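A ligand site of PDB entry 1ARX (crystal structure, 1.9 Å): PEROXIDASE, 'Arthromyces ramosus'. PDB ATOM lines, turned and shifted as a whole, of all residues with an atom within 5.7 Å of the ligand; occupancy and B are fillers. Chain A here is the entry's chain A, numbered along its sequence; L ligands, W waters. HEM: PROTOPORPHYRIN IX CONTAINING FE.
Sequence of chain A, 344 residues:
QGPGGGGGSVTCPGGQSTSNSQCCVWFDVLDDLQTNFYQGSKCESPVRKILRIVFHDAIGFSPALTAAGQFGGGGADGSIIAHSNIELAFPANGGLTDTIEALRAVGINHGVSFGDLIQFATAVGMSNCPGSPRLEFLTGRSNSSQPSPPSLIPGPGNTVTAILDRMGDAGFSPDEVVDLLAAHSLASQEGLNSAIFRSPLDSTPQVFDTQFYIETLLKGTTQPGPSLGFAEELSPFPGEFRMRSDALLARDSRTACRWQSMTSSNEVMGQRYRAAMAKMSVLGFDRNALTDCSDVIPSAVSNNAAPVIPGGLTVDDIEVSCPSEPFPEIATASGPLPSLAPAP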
ATOM      1  N   SER A  45     -24.404 -22.128  -8.694  1.00  0.00           N
ATOM      2  CA  SER A  45     -24.671 -22.941  -9.857  1.00  0.00           C
ATOM      3  C   SER A  45     -24.572 -22.259 -11.236  1.00  0.00           C
ATOM      4  O   SER A  45     -23.978 -22.932 -12.068  1.00  0.00           O
ATOM      5  CB  SER A  45     -26.034 -23.571  -9.658  1.00  0.00           C
ATOM      6  OG  SER A  45     -26.320 -24.512 -10.685  1.00  0.00           O
ATOM      7  N   VAL A  47     -22.493 -20.044 -12.506  1.00  0.00           N
ATOM      8  CA  VAL A  47     -21.057 -20.058 -12.841  1.00  0.00           C
ATOM      9  C   VAL A  47     -20.604 -21.482 -13.197  1.00  0.00           C
ATOM     10  O   VAL A  47     -19.949 -21.733 -14.205  1.00  0.00           O
ATOM     11  CB  VAL A  47     -20.224 -19.549 -11.624  1.00  0.00           C
ATOM     12  CG1 VAL A  47     -18.711 -19.645 -11.866  1.00  0.00           C
ATOM     13  CG2 VAL A  47     -20.603 -18.110 -11.349  1.00  0.00           C
ATOM     14  N   ARG A  48     -20.935 -22.480 -12.374  1.00  0.00           N
ATOM     15  CA  ARG A  48     -20.539 -23.865 -12.605  1.00  0.00           C
ATOM     16  C   ARG A  48     -21.046 -24.428 -13.896  1.00  0.00           C
ATOM     17  O   ARG A  48     -20.302 -25.054 -14.638  1.00  0.00           O
ATOM     18  CB  ARG A  48     -21.035 -24.700 -11.475  1.00  0.00           C
ATOM     19  CG  ARG A  48     -20.380 -24.394 -10.153  1.00  0.00           C
ATOM     20  CD  ARG A  48     -20.912 -25.497  -9.301  1.00  0.00           C
ATOM     21  NE  ARG A  48     -21.267 -24.837  -8.133  1.00  0.00           N
ATOM     22  CZ  ARG A  48     -22.412 -24.926  -7.536  1.00  0.00           C
ATOM     23  NH1 ARG A  48     -23.466 -25.690  -7.910  1.00  0.00           N
ATOM     24  NH2 ARG A  48     -22.436 -24.054  -6.553  1.00  0.00           N
ATOM     25  N   LYS A  49     -22.290 -24.141 -14.239  1.00  0.00           N
ATOM     26  CA  LYS A  49     -22.919 -24.537 -15.481  1.00  0.00           C
ATOM     27  C   LYS A  49     -22.233 -23.888 -16.675  1.00  0.00           C
ATOM     28  O   LYS A  49     -21.970 -24.520 -17.696  1.00  0.00           O
ATOM     29  CB  LYS A  49     -24.398 -24.126 -15.440  1.00  0.00           C
ATOM     30  CG  LYS A  49     -25.274 -24.781 -14.383  1.00  0.00           C
ATOM     31  CD  LYS A  49     -25.434 -26.232 -14.728  1.00  0.00           C
ATOM     32  CE  LYS A  49     -26.322 -26.963 -13.745  1.00  0.00           C
ATOM     33  NZ  LYS A  49     -26.497 -28.329 -14.190  1.00  0.00           N
ATOM     34  N   LEU A  51     -19.172 -22.877 -16.799  1.00  0.00           N
ATOM     35  CA  LEU A  51     -17.863 -23.455 -17.007  1.00  0.00           C
ATOM     36  C   LEU A  51     -18.002 -24.756 -17.793  1.00  0.00           C
ATOM     37  O   LEU A  51     -17.116 -25.061 -18.607  1.00  0.00           O
ATOM     38  CB  LEU A  51     -17.169 -23.685 -15.641  1.00  0.00           C
ATOM     39  CG  LEU A  51     -16.530 -22.467 -14.979  1.00  0.00           C
ATOM     40  CD1 LEU A  51     -16.106 -22.741 -13.579  1.00  0.00           C
ATOM     41  CD2 LEU A  51     -15.309 -22.078 -15.780  1.00  0.00           C
ATOM     42  N   ARG A  52     -19.081 -25.552 -17.629  1.00  0.00           N
ATOM     43  CA  ARG A  52     -19.261 -26.769 -18.429  1.00  0.00           C
ATOM     44  C   ARG A  52     -19.523 -26.364 -19.877  1.00  0.00           C
ATOM     45  O   ARG A  52     -18.917 -26.945 -20.777  1.00  0.00           O
ATOM     46  CB  ARG A  52     -20.460 -27.608 -17.992  1.00  0.00           C
ATOM     47  CG  ARG A  52     -20.216 -28.384 -16.734  1.00  0.00           C
ATOM     48  CD  ARG A  52     -21.410 -29.243 -16.351  1.00  0.00           C
ATOM     49  NE  ARG A  52     -21.671 -30.256 -17.375  1.00  0.00           N
ATOM     50  CZ  ARG A  52     -22.890 -30.785 -17.507  1.00  0.00           C
ATOM     51  NH1 ARG A  52     -23.914 -30.425 -16.716  1.00  0.00           N
ATOM     52  NH2 ARG A  52     -23.097 -31.667 -18.458  1.00  0.00           N
ATOM     53  N   VAL A  54     -18.622 -23.506 -21.637  1.00  0.00           N
ATOM     54  CA  VAL A  54     -17.467 -23.007 -22.373  1.00  0.00           C
ATOM     55  C   VAL A  54     -16.621 -24.202 -22.836  1.00  0.00           C
ATOM     56  O   VAL A  54     -16.254 -24.247 -24.011  1.00  0.00           O
ATOM     57  CB  VAL A  54     -16.735 -22.016 -21.407  1.00  0.00           C
ATOM     58  CG1 VAL A  54     -15.937 -22.716 -20.297  1.00  0.00           C
ATOM     59  CG2 VAL A  54     -15.832 -21.148 -22.235  1.00  0.00           C
ATOM     60  N   PHE A  55     -16.406 -25.240 -21.984  1.00  0.00           N
ATOM     61  CA  PHE A  55     -15.661 -26.434 -22.355  1.00  0.00           C
ATOM     62  C   PHE A  55     -16.374 -27.155 -23.473  1.00  0.00           C
ATOM     63  O   PHE A  55     -15.812 -27.314 -24.559  1.00  0.00           O
ATOM     64  CB  PHE A  55     -15.496 -27.412 -21.158  1.00  0.00           C
ATOM     65  CG  PHE A  55     -14.807 -28.766 -21.416  1.00  0.00           C
ATOM     66  CD1 PHE A  55     -13.728 -28.894 -22.296  1.00  0.00           C
ATOM     67  CD2 PHE A  55     -15.247 -29.895 -20.759  1.00  0.00           C
ATOM     68  CE1 PHE A  55     -13.123 -30.133 -22.505  1.00  0.00           C
ATOM     69  CE2 PHE A  55     -14.632 -31.123 -20.951  1.00  0.00           C
ATOM     70  CZ  PHE A  55     -13.573 -31.244 -21.830  1.00  0.00           C
ATOM     71  N   PRO A 154     -15.114 -35.503 -24.004  1.00  0.00           N
ATOM     72  CA  PRO A 154     -14.590 -36.459 -23.019  1.00  0.00           C
ATOM     73  C   PRO A 154     -15.675 -36.792 -22.000  1.00  0.00           C
ATOM     74  O   PRO A 154     -16.421 -35.895 -21.594  1.00  0.00           O
ATOM     75  CB  PRO A 154     -13.397 -35.731 -22.416  1.00  0.00           C
ATOM     76  CG  PRO A 154     -12.901 -34.895 -23.571  1.00  0.00           C
ATOM     77  CD  PRO A 154     -14.201 -34.363 -24.144  1.00  0.00           C
ATOM     78  N   GLY A 155     -15.823 -38.049 -21.585  1.00  0.00           N
ATOM     79  CA  GLY A 155     -16.805 -38.420 -20.594  1.00  0.00           C
ATOM     80  C   GLY A 155     -16.106 -38.952 -19.366  1.00  0.00           C
ATOM     81  O   GLY A 155     -14.939 -39.373 -19.447  1.00  0.00           O
ATOM     82  N   PRO A 156     -16.766 -38.995 -18.192  1.00  0.00           N
ATOM     83  CA  PRO A 156     -16.195 -39.475 -16.942  1.00  0.00           C
ATOM     84  C   PRO A 156     -15.843 -40.964 -16.909  1.00  0.00           C
ATOM     85  O   PRO A 156     -15.042 -41.377 -16.059  1.00  0.00           O
ATOM     86  CB  PRO A 156     -17.223 -39.075 -15.891  1.00  0.00           C
ATOM     87  CG  PRO A 156     -18.541 -39.285 -16.619  1.00  0.00           C
ATOM     88  CD  PRO A 156     -18.193 -38.665 -17.998  1.00  0.00           C
ATOM     89  N   ILE A 163      -9.108 -39.883 -23.124  1.00  0.00           N
ATOM     90  CA  ILE A 163      -9.200 -38.461 -22.806  1.00  0.00           C
ATOM     91  C   ILE A 163      -7.981 -37.781 -23.389  1.00  0.00           C
ATOM     92  O   ILE A 163      -8.132 -36.802 -24.116  1.00  0.00           O
ATOM     93  CB  ILE A 163      -9.262 -38.265 -21.271  1.00  0.00           C
ATOM     94  CG1 ILE A 163     -10.627 -38.789 -20.779  1.00  0.00           C
ATOM     95  CG2 ILE A 163      -9.050 -36.779 -20.897  1.00  0.00           C
ATOM     96  CD1 ILE A 163     -10.700 -39.027 -19.238  1.00  0.00           C
ATOM     97  N   MET A 167      -8.308 -34.893 -26.269  1.00  0.00           N
ATOM     98  CA  MET A 167      -7.840 -33.568 -25.876  1.00  0.00           C
ATOM     99  C   MET A 167      -6.634 -33.153 -26.691  1.00  0.00           C
ATOM    100  O   MET A 167      -6.528 -31.994 -27.096  1.00  0.00           O
ATOM    101  CB  MET A 167      -7.482 -33.559 -24.392  1.00  0.00           C
ATOM    102  CG  MET A 167      -8.695 -33.597 -23.488  1.00  0.00           C
ATOM    103  SD  MET A 167      -9.849 -32.215 -23.646  1.00  0.00           S
ATOM    104  CE  MET A 167      -9.098 -31.007 -22.585  1.00  0.00           C
ATOM    105  N   VAL A 177      -4.270 -30.576 -19.992  1.00  0.00           N
ATOM    106  CA  VAL A 177      -5.506 -31.277 -19.623  1.00  0.00           C
ATOM    107  C   VAL A 177      -5.612 -31.103 -18.125  1.00  0.00           C
ATOM    108  O   VAL A 177      -6.642 -30.652 -17.627  1.00  0.00           O
ATOM    109  CB  VAL A 177      -5.424 -32.791 -20.028  1.00  0.00           C
ATOM    110  CG1 VAL A 177      -6.689 -33.571 -19.627  1.00  0.00           C
ATOM    111  CG2 VAL A 177      -5.302 -32.895 -21.534  1.00  0.00           C
ATOM    112  N   LEU A 180      -6.453 -27.431 -17.112  1.00  0.00           N
ATOM    113  CA  LEU A 180      -7.848 -27.167 -17.438  1.00  0.00           C
ATOM    114  C   LEU A 180      -8.787 -27.699 -16.360  1.00  0.00           C
ATOM    115  O   LEU A 180      -9.845 -27.122 -16.071  1.00  0.00           O
ATOM    116  CB  LEU A 180      -8.177 -27.811 -18.753  1.00  0.00           C
ATOM    117  CG  LEU A 180      -8.679 -27.042 -19.942  1.00  0.00           C
ATOM    118  CD1 LEU A 180      -8.315 -25.566 -19.877  1.00  0.00           C
ATOM    119  CD2 LEU A 180      -8.084 -27.734 -21.159  1.00  0.00           C
ATOM    120  N   LEU A 181      -8.412 -28.809 -15.735  1.00  0.00           N
ATOM    121  CA  LEU A 181      -9.238 -29.395 -14.686  1.00  0.00           C
ATOM    122  C   LEU A 181      -9.245 -28.622 -13.383  1.00  0.00           C
ATOM    123  O   LEU A 181      -9.894 -29.059 -12.426  1.00  0.00           O
ATOM    124  CB  LEU A 181      -8.792 -30.814 -14.409  1.00  0.00           C
ATOM    125  CG  LEU A 181      -9.332 -31.781 -15.446  1.00  0.00           C
ATOM    126  CD1 LEU A 181      -8.675 -33.110 -15.289  1.00  0.00           C
ATOM    127  CD2 LEU A 181     -10.823 -31.921 -15.276  1.00  0.00           C
ATOM    128  N   ALA A 183     -10.902 -26.102 -13.070  1.00  0.00           N
ATOM    129  CA  ALA A 183     -12.295 -25.687 -12.945  1.00  0.00           C
ATOM    130  C   ALA A 183     -13.139 -26.618 -12.069  1.00  0.00           C
ATOM    131  O   ALA A 183     -14.155 -26.178 -11.494  1.00  0.00           O
ATOM    132  CB  ALA A 183     -12.980 -25.627 -14.293  1.00  0.00           C
ATOM    133  N   HIS A 184     -12.661 -27.851 -11.801  1.00  0.00           N
ATOM    134  CA  HIS A 184     -13.362 -28.760 -10.913  1.00  0.00           C
ATOM    135  C   HIS A 184     -13.191 -28.331  -9.445  1.00  0.00           C
ATOM    136  O   HIS A 184     -13.720 -28.931  -8.496  1.00  0.00           O
ATOM    137  CB  HIS A 184     -12.851 -30.204 -11.166  1.00  0.00           C
ATOM    138  CG  HIS A 184     -13.514 -30.953 -12.335  1.00  0.00           C
ATOM    139  ND1 HIS A 184     -13.476 -32.328 -12.522  1.00  0.00           N
ATOM    140  CD2 HIS A 184     -14.274 -30.366 -13.334  1.00  0.00           C
ATOM    141  CE1 HIS A 184     -14.225 -32.577 -13.614  1.00  0.00           C
ATOM    142  NE2 HIS A 184     -14.700 -31.468 -14.099  1.00  0.00           N
ATOM    143  N   LEU A 186     -14.449 -25.529  -8.614  1.00  0.00           N
ATOM    144  CA  LEU A 186     -15.709 -24.838  -8.384  1.00  0.00           C
ATOM    145  C   LEU A 186     -16.733 -25.802  -8.988  1.00  0.00           C
ATOM    146  O   LEU A 186     -17.370 -25.485  -9.981  1.00  0.00           O
ATOM    147  CB  LEU A 186     -15.812 -23.487  -9.138  1.00  0.00           C
ATOM    148  CG  LEU A 186     -15.175 -22.113  -8.801  1.00  0.00           C
ATOM    149  CD1 LEU A 186     -14.844 -21.960  -7.320  1.00  0.00           C
ATOM    150  CD2 LEU A 186     -13.973 -21.958  -9.670  1.00  0.00           C
ATOM    151  N   ALA A 187     -16.964 -26.964  -8.422  1.00  0.00           N
ATOM    152  CA  ALA A 187     -17.802 -27.936  -9.103  1.00  0.00           C
ATOM    153  C   ALA A 187     -18.578 -28.898  -8.263  1.00  0.00           C
ATOM    154  O   ALA A 187     -18.209 -29.167  -7.119  1.00  0.00           O
ATOM    155  CB  ALA A 187     -16.956 -28.790 -10.032  1.00  0.00           C
ATOM    156  N   SER A 188     -19.604 -29.491  -8.835  1.00  0.00           N
ATOM    157  CA  SER A 188     -20.377 -30.496  -8.141  1.00  0.00           C
ATOM    158  C   SER A 188     -20.978 -31.340  -9.247  1.00  0.00           C
ATOM    159  O   SER A 188     -20.771 -31.036 -10.434  1.00  0.00           O
ATOM    160  CB  SER A 188     -21.502 -29.833  -7.342  1.00  0.00           C
ATOM    161  OG  SER A 188     -22.539 -29.269  -8.121  1.00  0.00           O
ATOM    162  N   GLN A 189     -21.717 -32.405  -8.929  1.00  0.00           N
ATOM    163  CA  GLN A 189     -22.399 -33.124 -10.006  1.00  0.00           C
ATOM    164  C   GLN A 189     -23.889 -33.101  -9.670  1.00  0.00           C
ATOM    165  O   GLN A 189     -24.295 -33.019  -8.493  1.00  0.00           O
ATOM    166  CB  GLN A 189     -21.901 -34.579 -10.120  1.00  0.00           C
ATOM    167  CG  GLN A 189     -22.075 -35.410  -8.855  1.00  0.00           C
ATOM    168  CD  GLN A 189     -23.458 -36.047  -8.717  1.00  0.00           C
ATOM    169  OE1 GLN A 189     -24.089 -36.360  -9.733  1.00  0.00           O
ATOM    170  NE2 GLN A 189     -23.948 -36.215  -7.505  1.00  0.00           N
ATOM    171  N   GLU A 190     -24.708 -33.161 -10.704  1.00  0.00           N
ATOM    172  CA  GLU A 190     -26.151 -33.227 -10.526  1.00  0.00           C
ATOM    173  C   GLU A 190     -26.718 -34.502 -11.115  1.00  0.00           C
ATOM    174  O   GLU A 190     -27.614 -35.122 -10.526  1.00  0.00           O
ATOM    175  CB  GLU A 190     -26.844 -32.088 -11.214  1.00  0.00           C
ATOM    176  CG  GLU A 190     -26.585 -30.808 -10.476  1.00  0.00           C
ATOM    177  CD  GLU A 190     -27.249 -29.567 -11.064  1.00  0.00           C
ATOM    178  OE1 GLU A 190     -27.962 -29.669 -12.053  1.00  0.00           O
ATOM    179  OE2 GLU A 190     -27.041 -28.489 -10.514  1.00  0.00           O
ATOM    180  N   GLY A 191     -26.193 -34.863 -12.291  1.00  0.00           N
ATOM    181  CA  GLY A 191     -26.678 -36.006 -13.049  1.00  0.00           C
ATOM    182  C   GLY A 191     -25.954 -37.334 -12.918  1.00  0.00           C
ATOM    183  O   GLY A 191     -26.476 -38.308 -13.428  1.00  0.00           O
ATOM    184  N   LEU A 192     -24.789 -37.479 -12.290  1.00  0.00           N
ATOM    185  CA  LEU A 192     -24.128 -38.769 -12.184  1.00  0.00           C
ATOM    186  C   LEU A 192     -24.712 -39.594 -11.052  1.00  0.00           C
ATOM    187  O   LEU A 192     -24.783 -40.827 -11.110  1.00  0.00           O
ATOM    188  CB  LEU A 192     -22.661 -38.475 -11.980  1.00  0.00           C
ATOM    189  CG  LEU A 192     -21.600 -38.592 -13.088  1.00  0.00           C
ATOM    190  CD1 LEU A 192     -22.115 -38.316 -14.491  1.00  0.00           C
ATOM    191  CD2 LEU A 192     -20.507 -37.640 -12.687  1.00  0.00           C
ATOM    192  N   LEU A 201     -17.078 -31.531  -5.642  1.00  0.00           N
ATOM    193  CA  LEU A 201     -15.910 -32.281  -6.071  1.00  0.00           C
ATOM    194  C   LEU A 201     -14.729 -31.895  -5.190  1.00  0.00           C
ATOM    195  O   LEU A 201     -13.739 -32.622  -5.136  1.00  0.00           O
ATOM    196  CB  LEU A 201     -15.651 -31.999  -7.563  1.00  0.00           C
ATOM    197  CG  LEU A 201     -16.216 -33.020  -8.615  1.00  0.00           C
ATOM    198  CD1 LEU A 201     -17.593 -33.577  -8.231  1.00  0.00           C
ATOM    199  CD2 LEU A 201     -16.300 -32.305  -9.965  1.00  0.00           C
ATOM    200  N   MET A 243     -15.394 -38.523  -9.320  1.00  0.00           N
ATOM    201  CA  MET A 243     -15.654 -39.219 -10.569  1.00  0.00           C
ATOM    202  C   MET A 243     -14.370 -39.941 -11.023  1.00  0.00           C
ATOM    203  O   MET A 243     -13.230 -39.535 -10.742  1.00  0.00           O
ATOM    204  CB  MET A 243     -16.128 -38.259 -11.685  1.00  0.00           C
ATOM    205  CG  MET A 243     -15.122 -37.307 -12.276  1.00  0.00           C
ATOM    206  SD  MET A 243     -15.803 -36.170 -13.521  1.00  0.00           S
ATOM    207  CE  MET A 243     -16.493 -35.043 -12.319  1.00  0.00           C
ATOM    208  N   SER A 245     -12.743 -40.410 -13.945  1.00  0.00           N
ATOM    209  CA  SER A 245     -11.722 -39.787 -14.786  1.00  0.00           C
ATOM    210  C   SER A 245     -10.755 -38.958 -13.960  1.00  0.00           C
ATOM    211  O   SER A 245      -9.546 -39.053 -14.161  1.00  0.00           O
ATOM    212  CB  SER A 245     -12.389 -38.921 -15.855  1.00  0.00           C
ATOM    213  OG  SER A 245     -13.396 -38.040 -15.384  1.00  0.00           O
ATOM    214  N   LEU A 249      -6.707 -39.690 -13.590  1.00  0.00           N
ATOM    215  CA  LEU A 249      -5.719 -38.712 -14.040  1.00  0.00           C
ATOM    216  C   LEU A 249      -4.803 -38.316 -12.897  1.00  0.00           C
ATOM    217  O   LEU A 249      -3.618 -38.084 -13.102  1.00  0.00           O
ATOM    218  CB  LEU A 249      -6.431 -37.458 -14.639  1.00  0.00           C
ATOM    219  CG  LEU A 249      -7.153 -37.632 -15.997  1.00  0.00           C
ATOM    220  CD1 LEU A 249      -8.171 -36.538 -16.257  1.00  0.00           C
ATOM    221  CD2 LEU A 249      -6.107 -37.666 -17.066  1.00  0.00           C
ATOM    222  N   TYR A 273      -3.994 -22.247 -15.309  1.00  0.00           N
ATOM    223  CA  TYR A 273      -5.383 -22.302 -15.696  1.00  0.00           C
ATOM    224  C   TYR A 273      -5.711 -21.204 -16.707  1.00  0.00           C
ATOM    225  O   TYR A 273      -6.280 -21.498 -17.759  1.00  0.00           O
ATOM    226  CB  TYR A 273      -6.284 -22.156 -14.450  1.00  0.00           C
ATOM    227  CG  TYR A 273      -7.781 -22.169 -14.791  1.00  0.00           C
ATOM    228  CD1 TYR A 273      -8.382 -23.347 -15.247  1.00  0.00           C
ATOM    229  CD2 TYR A 273      -8.512 -21.007 -14.614  1.00  0.00           C
ATOM    230  CE1 TYR A 273      -9.727 -23.370 -15.526  1.00  0.00           C
ATOM    231  CE2 TYR A 273      -9.856 -21.031 -14.893  1.00  0.00           C
ATOM    232  CZ  TYR A 273     -10.443 -22.207 -15.341  1.00  0.00           C
ATOM    233  OH  TYR A 273     -11.806 -22.214 -15.524  1.00  0.00           O
ATOM    234  N   MET A 277      -7.033 -21.783 -20.453  1.00  0.00           N
ATOM    235  CA  MET A 277      -8.296 -21.193 -20.896  1.00  0.00           C
ATOM    236  C   MET A 277      -8.159 -20.215 -22.069  1.00  0.00           C
ATOM    237  O   MET A 277      -9.045 -20.164 -22.948  1.00  0.00           O
ATOM    238  CB  MET A 277      -8.981 -20.426 -19.770  1.00  0.00           C
ATOM    239  CG  MET A 277      -9.549 -21.402 -18.749  1.00  0.00           C
ATOM    240  SD  MET A 277     -10.851 -22.535 -19.327  1.00  0.00           S
ATOM    241  CE  MET A 277     -12.260 -21.468 -19.300  1.00  0.00           C
ATOM    242  N   MET A 280      -7.981 -22.410 -25.197  1.00  0.00           N
ATOM    243  CA  MET A 280      -9.265 -23.019 -25.489  1.00  0.00           C
ATOM    244  C   MET A 280     -10.239 -22.006 -26.053  1.00  0.00           C
ATOM    245  O   MET A 280     -11.041 -22.368 -26.922  1.00  0.00           O
ATOM    246  CB  MET A 280      -9.813 -23.628 -24.205  1.00  0.00           C
ATOM    247  CG  MET A 280     -11.078 -24.412 -24.499  1.00  0.00           C
ATOM    248  SD  MET A 280     -11.606 -25.467 -23.165  1.00  0.00           S
ATOM    249  CE  MET A 280     -12.430 -24.227 -22.204  1.00  0.00           C
HETATM  250  CHA HEM L   1     -18.726 -31.108 -13.854  1.00  0.00           C
HETATM  251  CHB HEM L   1     -16.556 -34.394 -16.533  1.00  0.00           C
HETATM  252  CHC HEM L   1     -13.283 -31.177 -17.854  1.00  0.00           C
HETATM  253  CHD HEM L   1     -15.823 -27.770 -15.653  1.00  0.00           C
HETATM  254  C1A HEM L   1     -18.416 -32.275 -14.462  1.00  0.00           C
HETATM  255  C2A HEM L   1     -19.241 -33.451 -14.407  1.00  0.00           C
HETATM  256  C3A HEM L   1     -18.625 -34.393 -15.142  1.00  0.00           C
HETATM  257  C4A HEM L   1     -17.443 -33.777 -15.691  1.00  0.00           C
HETATM  258  CMA HEM L   1     -19.026 -35.830 -15.294  1.00  0.00           C
HETATM  259  CAA HEM L   1     -20.579 -33.547 -13.701  1.00  0.00           C
HETATM  260  CBA HEM L   1     -21.779 -33.054 -14.519  1.00  0.00           C
HETATM  261  CGA HEM L   1     -23.108 -33.267 -13.783  1.00  0.00           C
HETATM  262  O1A HEM L   1     -23.728 -32.322 -13.314  1.00  0.00           O
HETATM  263  O2A HEM L   1     -23.555 -34.392 -13.633  1.00  0.00           O
HETATM  264  C1B HEM L   1     -15.425 -33.817 -17.038  1.00  0.00           C
HETATM  265  C2B HEM L   1     -14.415 -34.552 -17.754  1.00  0.00           C
HETATM  266  C3B HEM L   1     -13.422 -33.686 -18.093  1.00  0.00           C
HETATM  267  C4B HEM L   1     -13.860 -32.394 -17.552  1.00  0.00           C
HETATM  268  CMB HEM L   1     -14.400 -36.039 -18.051  1.00  0.00           C
HETATM  269  CAB HEM L   1     -12.227 -34.096 -18.677  1.00  0.00           C
HETATM  270  CBB HEM L   1     -11.369 -33.331 -19.547  1.00  0.00           C
HETATM  271  C1C HEM L   1     -13.774 -29.957 -17.473  1.00  0.00           C
HETATM  272  C2C HEM L   1     -13.278 -28.706 -17.976  1.00  0.00           C
HETATM  273  C3C HEM L   1     -14.064 -27.716 -17.424  1.00  0.00           C
HETATM  274  C4C HEM L   1     -15.001 -28.400 -16.555  1.00  0.00           C
HETATM  275  CMC HEM L   1     -12.071 -28.557 -18.902  1.00  0.00           C
HETATM  276  CAC HEM L   1     -14.086 -26.354 -17.687  1.00  0.00           C
HETATM  277  CBC HEM L   1     -12.929 -25.496 -17.799  1.00  0.00           C
HETATM  278  C1D HEM L   1     -16.691 -28.434 -14.784  1.00  0.00           C
HETATM  279  C2D HEM L   1     -17.575 -27.770 -13.833  1.00  0.00           C
HETATM  280  C3D HEM L   1     -18.438 -28.695 -13.394  1.00  0.00           C
HETATM  281  C4D HEM L   1     -18.048 -29.929 -14.004  1.00  0.00           C
HETATM  282  CMD HEM L   1     -17.410 -26.361 -13.328  1.00  0.00           C
HETATM  283  CAD HEM L   1     -19.522 -28.507 -12.355  1.00  0.00           C
HETATM  284  CBD HEM L   1     -20.933 -28.225 -12.856  1.00  0.00           C
HETATM  285  CGD HEM L   1     -21.974 -28.057 -11.745  1.00  0.00           C
HETATM  286  O1D HEM L   1     -23.144 -27.930 -12.050  1.00  0.00           O
HETATM  287  O2D HEM L   1     -21.662 -28.074 -10.556  1.00  0.00           O
HETATM  288  NA  HEM L   1     -17.322 -32.474 -15.269  1.00  0.00           N
HETATM  289  NB  HEM L   1     -15.054 -32.514 -16.841  1.00  0.00           N
HETATM  290  NC  HEM L   1     -14.850 -29.778 -16.622  1.00  0.00           N
HETATM  291  ND  HEM L   1     -16.942 -29.780 -14.814  1.00  0.00           N
HETATM  292 FE   HEM L   1     -15.955 -31.161 -15.745  1.00  0.00          FE
HETATM  293  O   HOH W   1     -24.023 -29.738 -13.907  1.00  0.00           O
HETATM  294  O   HOH W   2     -26.127 -31.927 -14.995  1.00  0.00           O
HETATM  295  O   HOH W   3     -17.123 -33.516 -20.069  1.00  0.00           O
HETATM  296  O   HOH W   4     -12.038 -35.623 -15.489  1.00  0.00           O
HETATM  297  O   HOH W   5     -23.640 -35.944 -16.092  1.00  0.00           O
HETATM  298  O   HOH W   6     -24.756 -26.738 -10.344  1.00  0.00           O
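The guanidinium group (NH1) of Arg 52 lies within salt-bridge range of an oxygen (O1A) of the ligand (3.9 Å).
The side-chain hydroxyl (OG) of Ser 188 sits at hydrogen-bond distance from an oxygen (O2D) of the ligand (2.9 Å).
The side-chain amino group (NZ) of Lys 49 lies within salt-bridge range of an oxygen (O1D) of the ligand.
An oxygen (O2A) of the ligand is in hydrogen-bond range of the backbone NH of Gly 191 (3.0 Å).
The backbone carbonyl oxygen (O) of Ser 188 sits close to an oxygen (O2D) of the ligand (3.1 Å).
NH1 of Arg 48 lies within salt-bridge range of O2D of the ligand.
The backbone NH of Ser 188 is in hydrogen-bond range of an oxygen (O2D) of the ligand (3.0 Å).
The backbone NH of Glu 190 sits at hydrogen-bond distance from an oxygen (O1A) of the ligand, at 2.9 Å.
A ring nitrogen (NE2) of His 184 binds an iron atom (FE) of the ligand (2.1 Å).
Water W6 lies within hydrogen-bond range of O1D of the ligand, OG of Ser 45, OE2 of Glu 190 and NH1 of Arg 48.
Water W1 lies within hydrogen-bond range of O1A of the ligand (2.7 Å), NZ of Lys 49 (2.9 Å) and NH1 of Arg 52 (2.9 Å).
Water W2 lies within hydrogen-bond range of O1A of the ligand and NH1 of Arg 52.
The backbone carbonyl oxygen (O) of Ala 187 sits at hydrogen-bond distance from the backbone NH (N) of Leu 201, 3.0 Å away.
The backbone NH (N) of Leu 192 sits at hydrogen-bond distance from the side-chain amide oxygen (OE1) of Gln 189, at 2.9 Å.
N of Ser 245 lies within hydrogen-bond range of O of Pro 156, at 3.3 Å.
The side-chain amino group (NZ) of Lys 49 is in salt-bridge range of the side-chain carboxylate (OE1) of Glu 190, at 2.9 Å.
OG of Ser 245 is in hydrogen-bond range of SD of Met 243, 3.6 Å away.
Leu 51 touches the ligand (O to CAC, 3.4 Å).
Phe 55 touches the ligand.
Gly 155 touches the ligand (C to CMB, 3.6 Å).
CG of Pro 156 touches CMA of the ligand, 3.7 Å away.
Leu 180 touches the ligand.
Leu 181 touches the ligand.
Ala 183 touches the ligand (CB to CBC, 3.5 Å).
O of Leu 186 touches CMD of the ligand, at 3.5 Å.
CB of Ala 187 touches CAD of the ligand (3.5 Å).
Gln 189 touches the ligand (CA to O1A, 3.7 Å).
CD2 of Leu 192 touches CMA of the ligand, at 3.5 Å.
Met 243 touches the ligand.
OG of Ser 245 touches CMB of the ligand, at 3.5 Å.
Met 277 touches the ligand (SD to CBC, 3.9 Å).
Hydrophobic or aromatic side chains that line the ligand: Leu 51, Phe 55, Pro 156, Leu 180, Leu 181, Ala 183, His 184, Ala 187, Leu 192, Met 243 and Met 277.
Within 4 Å of the ligand: Arg 48, Lys 49, Leu 51, Arg 52, Phe 55, Gly 155, Pro 156, Leu 180, Leu 181, Ala 183, His 184, Leu 186, Ala 187, Ser 188, Gln 189, Glu 190, Gly 191, Leu 192, Met 243, Ser 245 and Met 277.
Along chain A the residues within 4 Å of the ligand span positions 48 to 277.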
